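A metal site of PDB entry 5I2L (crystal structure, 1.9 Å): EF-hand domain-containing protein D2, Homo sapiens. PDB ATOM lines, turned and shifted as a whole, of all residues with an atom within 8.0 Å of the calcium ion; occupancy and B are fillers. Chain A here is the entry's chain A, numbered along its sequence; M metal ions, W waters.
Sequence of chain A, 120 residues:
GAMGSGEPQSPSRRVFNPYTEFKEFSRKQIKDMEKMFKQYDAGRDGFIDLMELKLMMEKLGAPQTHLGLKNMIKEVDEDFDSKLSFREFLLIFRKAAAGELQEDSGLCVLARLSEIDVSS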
ATOM      1  N   PHE A  47      -4.893  -6.095  17.805  1.00  0.00           N
ATOM      2  CA  PHE A  47      -3.430  -6.102  17.803  1.00  0.00           C
ATOM      3  C   PHE A  47      -2.940  -5.690  16.450  1.00  0.00           C
ATOM      4  O   PHE A  47      -3.659  -5.781  15.483  1.00  0.00           O
ATOM      5  CB  PHE A  47      -2.904  -7.512  18.066  1.00  0.00           C
ATOM      6  CG  PHE A  47      -3.373  -8.094  19.359  1.00  0.00           C
ATOM      7  CD1 PHE A  47      -2.735  -7.764  20.542  1.00  0.00           C
ATOM      8  CD2 PHE A  47      -4.448  -8.965  19.395  1.00  0.00           C
ATOM      9  CE1 PHE A  47      -3.169  -8.268  21.746  1.00  0.00           C
ATOM     10  CE2 PHE A  47      -4.885  -9.493  20.606  1.00  0.00           C
ATOM     11  CZ  PHE A  47      -4.241  -9.148  21.772  1.00  0.00           C
ATOM     12  N   ILE A  48      -1.713  -5.217  16.379  1.00  0.00           N
ATOM     13  CA  ILE A  48      -1.080  -5.039  15.087  1.00  0.00           C
ATOM     14  C   ILE A  48       0.076  -6.016  15.027  1.00  0.00           C
ATOM     15  O   ILE A  48       1.032  -5.921  15.809  1.00  0.00           O
ATOM     16  CB  ILE A  48      -0.586  -3.596  14.880  1.00  0.00           C
ATOM     17  CG1 ILE A  48      -1.784  -2.697  14.641  1.00  0.00           C
ATOM     18  CG2 ILE A  48       0.351  -3.514  13.669  1.00  0.00           C
ATOM     19  CD1 ILE A  48      -1.408  -1.255  14.432  1.00  0.00           C
ATOM     20  N   ILE A  73       8.700  -4.031  16.620  1.00  0.00           N
ATOM     21  CA  ILE A  73       7.774  -4.690  17.545  1.00  0.00           C
ATOM     22  C   ILE A  73       8.476  -5.081  18.831  1.00  0.00           C
ATOM     23  O   ILE A  73       7.947  -4.849  19.911  1.00  0.00           O
ATOM     24  CB  ILE A  73       7.039  -5.894  16.888  1.00  0.00           C
ATOM     25  CG1 ILE A  73       6.011  -5.345  15.884  1.00  0.00           C
ATOM     26  CG2 ILE A  73       6.340  -6.758  17.945  1.00  0.00           C
ATOM     27  CD1 ILE A  73       5.404  -6.391  14.968  1.00  0.00           C
ATOM     28  N   VAL A  76       8.842  -2.583  21.853  1.00  0.00           N
ATOM     29  CA  VAL A  76       7.688  -2.247  22.695  1.00  0.00           C
ATOM     30  C   VAL A  76       6.794  -3.431  23.078  1.00  0.00           C
ATOM     31  O   VAL A  76       5.777  -3.243  23.747  1.00  0.00           O
ATOM     32  CB  VAL A  76       6.810  -1.126  22.062  1.00  0.00           C
ATOM     33  CG1 VAL A  76       7.556   0.188  22.005  1.00  0.00           C
ATOM     34  CG2 VAL A  76       6.294  -1.532  20.667  1.00  0.00           C
ATOM     35  N   ASP A  77       7.205  -4.643  22.684  1.00  0.00           N
ATOM     36  CA  ASP A  77       6.440  -5.864  22.893  1.00  0.00           C
ATOM     37  C   ASP A  77       6.620  -6.370  24.331  1.00  0.00           C
ATOM     38  O   ASP A  77       7.336  -7.340  24.568  1.00  0.00           O
ATOM     39  CB  ASP A  77       6.881  -6.914  21.872  1.00  0.00           C
ATOM     40  CG  ASP A  77       6.080  -8.174  21.971  1.00  0.00           C
ATOM     41  OD1 ASP A  77       5.018  -8.095  22.550  1.00  0.00           O
ATOM     42  OD2 ASP A  77       6.510  -9.226  21.515  1.00  0.00           O
ATOM     43  N   GLU A  78       5.966  -5.709  25.279  1.00  0.00           N
ATOM     44  CA  GLU A  78       6.151  -5.993  26.704  1.00  0.00           C
ATOM     45  C   GLU A  78       5.593  -7.338  27.169  1.00  0.00           C
ATOM     46  O   GLU A  78       6.002  -7.843  28.224  1.00  0.00           O
ATOM     47  CB  GLU A  78       5.590  -4.844  27.533  1.00  0.00           C
ATOM     48  CG  GLU A  78       6.437  -3.585  27.405  1.00  0.00           C
ATOM     49  CD  GLU A  78       6.179  -2.599  28.533  1.00  0.00           C
ATOM     50  OE1 GLU A  78       5.096  -2.656  29.138  1.00  0.00           O
ATOM     51  OE2 GLU A  78       7.063  -1.751  28.791  1.00  0.00           O
ATOM     52  N   ASP A  79       4.689  -7.948  26.411  1.00  0.00           N
ATOM     53  CA  ASP A  79       4.235  -9.279  26.794  1.00  0.00           C
ATOM     54  C   ASP A  79       4.689 -10.399  25.836  1.00  0.00           C
ATOM     55  O   ASP A  79       4.155 -11.506  25.834  1.00  0.00           O
ATOM     56  CB  ASP A  79       2.714  -9.328  27.085  1.00  0.00           C
ATOM     57  CG  ASP A  79       1.887  -9.085  25.871  1.00  0.00           C
ATOM     58  OD1 ASP A  79       2.504  -8.999  24.820  1.00  0.00           O
ATOM     59  OD2 ASP A  79       0.640  -8.987  25.952  1.00  0.00           O
ATOM     60  N   PHE A  80       5.673 -10.057  24.994  1.00  0.00           N
ATOM     61  CA  PHE A  80       6.423 -11.051  24.234  1.00  0.00           C
ATOM     62  C   PHE A  80       5.592 -11.977  23.330  1.00  0.00           C
ATOM     63  O   PHE A  80       5.920 -13.163  23.169  1.00  0.00           O
ATOM     64  CB  PHE A  80       7.306 -11.850  25.189  1.00  0.00           C
ATOM     65  CG  PHE A  80       8.212 -10.991  26.013  1.00  0.00           C
ATOM     66  CD1 PHE A  80       9.448 -10.588  25.518  1.00  0.00           C
ATOM     67  CD2 PHE A  80       7.818 -10.526  27.260  1.00  0.00           C
ATOM     68  CE1 PHE A  80      10.285  -9.783  26.268  1.00  0.00           C
ATOM     69  CE2 PHE A  80       8.636  -9.706  28.010  1.00  0.00           C
ATOM     70  CZ  PHE A  80       9.875  -9.324  27.514  1.00  0.00           C
ATOM     71  N   ASP A  81       4.515 -11.445  22.744  1.00  0.00           N
ATOM     72  CA  ASP A  81       3.667 -12.272  21.880  1.00  0.00           C
ATOM     73  C   ASP A  81       3.899 -11.931  20.392  1.00  0.00           C
ATOM     74  O   ASP A  81       3.191 -12.427  19.510  1.00  0.00           O
ATOM     75  CB  ASP A  81       2.190 -12.226  22.272  1.00  0.00           C
ATOM     76  CG  ASP A  81       1.544 -10.891  22.031  1.00  0.00           C
ATOM     77  OD1 ASP A  81       2.252 -10.004  21.546  1.00  0.00           O
ATOM     78  OD2 ASP A  81       0.334 -10.722  22.280  1.00  0.00           O
ATOM     79  N   SER A  82       4.890 -11.077  20.159  1.00  0.00           N
ATOM     80  CA  SER A  82       5.289 -10.641  18.803  1.00  0.00           C
ATOM     81  C   SER A  82       4.257  -9.841  17.988  1.00  0.00           C
ATOM     82  O   SER A  82       4.341  -9.765  16.765  1.00  0.00           O
ATOM     83  CB  SER A  82       5.800 -11.838  17.992  1.00  0.00           C
ATOM     84  OG  SER A  82       6.969 -12.395  18.581  1.00  0.00           O
ATOM     85  N   LYS A  83       3.268  -9.248  18.666  1.00  0.00           N
ATOM     86  CA  LYS A  83       2.340  -8.353  17.997  1.00  0.00           C
ATOM     87  C   LYS A  83       2.059  -7.202  18.955  1.00  0.00           C
ATOM     88  O   LYS A  83       2.431  -7.287  20.084  1.00  0.00           O
ATOM     89  CB  LYS A  83       1.047  -9.076  17.621  1.00  0.00           C
ATOM     90  CG  LYS A  83       0.323  -9.738  18.804  1.00  0.00           C
ATOM     91  CD  LYS A  83      -0.844 -10.604  18.312  1.00  0.00           C
ATOM     92  CE  LYS A  83      -1.459 -11.366  19.513  1.00  0.00           C
ATOM     93  NZ  LYS A  83      -2.724 -12.015  19.094  1.00  0.00           N
ATOM     94  N   LEU A  84       1.421  -6.125  18.514  1.00  0.00           N
ATOM     95  CA  LEU A  84       1.268  -4.939  19.372  1.00  0.00           C
ATOM     96  C   LEU A  84      -0.169  -4.752  19.830  1.00  0.00           C
ATOM     97  O   LEU A  84      -1.063  -4.675  19.008  1.00  0.00           O
ATOM     98  CB  LEU A  84       1.693  -3.693  18.609  1.00  0.00           C
ATOM     99  CG  LEU A  84       3.122  -3.670  18.089  1.00  0.00           C
ATOM    100  CD1 LEU A  84       3.391  -2.395  17.324  1.00  0.00           C
ATOM    101  CD2 LEU A  84       4.080  -3.816  19.242  1.00  0.00           C
ATOM    102  N   SER A  85      -0.391  -4.670  21.137  1.00  0.00           N
ATOM    103  CA  SER A  85      -1.706  -4.267  21.634  1.00  0.00           C
ATOM    104  C   SER A  85      -1.774  -2.756  21.525  1.00  0.00           C
ATOM    105  O   SER A  85      -0.777  -2.124  21.237  1.00  0.00           O
ATOM    106  CB  SER A  85      -1.847  -4.644  23.097  1.00  0.00           C
ATOM    107  OG  SER A  85      -0.890  -3.951  23.859  1.00  0.00           O
ATOM    108  N   PHE A  86      -2.927  -2.180  21.818  1.00  0.00           N
ATOM    109  CA  PHE A  86      -3.029  -0.714  21.765  1.00  0.00           C
ATOM    110  C   PHE A  86      -2.084  -0.064  22.778  1.00  0.00           C
ATOM    111  O   PHE A  86      -1.490   0.960  22.481  1.00  0.00           O
ATOM    112  CB  PHE A  86      -4.473  -0.257  21.992  1.00  0.00           C
ATOM    113  CG  PHE A  86      -4.642   1.251  21.932  1.00  0.00           C
ATOM    114  CD1 PHE A  86      -4.117   1.975  20.871  1.00  0.00           C
ATOM    115  CD2 PHE A  86      -5.345   1.922  22.919  1.00  0.00           C
ATOM    116  CE1 PHE A  86      -4.273   3.359  20.814  1.00  0.00           C
ATOM    117  CE2 PHE A  86      -5.507   3.304  22.871  1.00  0.00           C
ATOM    118  CZ  PHE A  86      -4.961   4.021  21.813  1.00  0.00           C
ATOM    119  N   ARG A  87      -1.957  -0.670  23.955  1.00  0.00           N
ATOM    120  CA  ARG A  87      -1.079  -0.135  25.000  1.00  0.00           C
ATOM    121  C   ARG A  87       0.363  -0.118  24.552  1.00  0.00           C
ATOM    122  O   ARG A  87       1.126   0.814  24.818  1.00  0.00           O
ATOM    123  CB  ARG A  87      -1.166  -0.991  26.264  1.00  0.00           C
ATOM    124  CG  ARG A  87      -0.173  -0.571  27.305  1.00  0.00           C
ATOM    125  CD  ARG A  87      -0.171  -1.484  28.514  1.00  0.00           C
ATOM    126  NE  ARG A  87       0.872  -1.019  29.422  1.00  0.00           N
ATOM    127  CZ  ARG A  87       2.136  -1.417  29.345  1.00  0.00           C
ATOM    128  NH1 ARG A  87       2.494  -2.321  28.435  1.00  0.00           N
ATOM    129  NH2 ARG A  87       3.021  -0.923  30.198  1.00  0.00           N
ATOM    130  N   GLU A  88       0.744  -1.161  23.830  1.00  0.00           N
ATOM    131  CA  GLU A  88       2.099  -1.217  23.342  1.00  0.00           C
ATOM    132  C   GLU A  88       2.332  -0.228  22.211  1.00  0.00           C
ATOM    133  O   GLU A  88       3.437   0.307  22.056  1.00  0.00           O
ATOM    134  CB  GLU A  88       2.453  -2.638  22.934  1.00  0.00           C
ATOM    135  CG  GLU A  88       2.580  -3.540  24.141  1.00  0.00           C
ATOM    136  CD  GLU A  88       2.530  -4.937  23.743  1.00  0.00           C
ATOM    137  OE1 GLU A  88       2.045  -5.169  22.603  1.00  0.00           O
ATOM    138  OE2 GLU A  88       2.956  -5.822  24.534  1.00  0.00           O
ATOM    139  N   PHE A  89       1.279   0.021  21.421  1.00  0.00           N
ATOM    140  CA  PHE A  89       1.331   1.045  20.385  1.00  0.00           C
ATOM    141  C   PHE A  89       1.566   2.438  21.028  1.00  0.00           C
ATOM    142  O   PHE A  89       2.358   3.241  20.531  1.00  0.00           O
ATOM    143  CB  PHE A  89       0.040   1.013  19.544  1.00  0.00           C
ATOM    144  CG  PHE A  89       0.085   1.863  18.297  1.00  0.00           C
ATOM    145  CD1 PHE A  89       0.882   1.508  17.215  1.00  0.00           C
ATOM    146  CD2 PHE A  89      -0.695   3.005  18.203  1.00  0.00           C
ATOM    147  CE1 PHE A  89       0.923   2.310  16.072  1.00  0.00           C
ATOM    148  CE2 PHE A  89      -0.662   3.798  17.065  1.00  0.00           C
ATOM    149  CZ  PHE A  89       0.149   3.452  16.008  1.00  0.00           C
HETATM  150 CA    CA M   1       2.493  -7.696  22.618  1.00  0.00          CA
HETATM  151  O   HOH W   1      -0.034  -8.114  22.531  1.00  0.00           O
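The backbone NH (N) of Glu 88 is in hydrogen-bond range of the side-chain hydroxyl (OG) of Ser 85.
The backbone NH (N) of Phe 80 lies close to the side-chain carboxylate (OD1) of Asp 77.
The side-chain carboxylate (OD2) of Asp 77 sits at hydrogen-bond distance from the backbone NH (N) of Ser 82.
OE2 of Glu 88 lies close to N of Glu 78 (3.1 Å).
Five residues have an atom within 4 Å of the calcium ion: Asp 77, Asp 79, Asp 81, Lys 83 and Glu 88.
Along chain A the residues within 4 Å of the calcium ion span positions 77 to 88.
The calcium ion is bound by OD1 of Asp 77 (2.6 Å), OD1 of Asp 81 (2.6 Å), OD1 of Asp 79 (2.6 Å), water W1 (2.6 Å), OE1 of Glu 88 (2.6 Å), O of Lys 83 (2.6 Å) and OE2 of Glu 88 (2.7 Å).
The calcium ion has seven donor atoms within binding distance.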
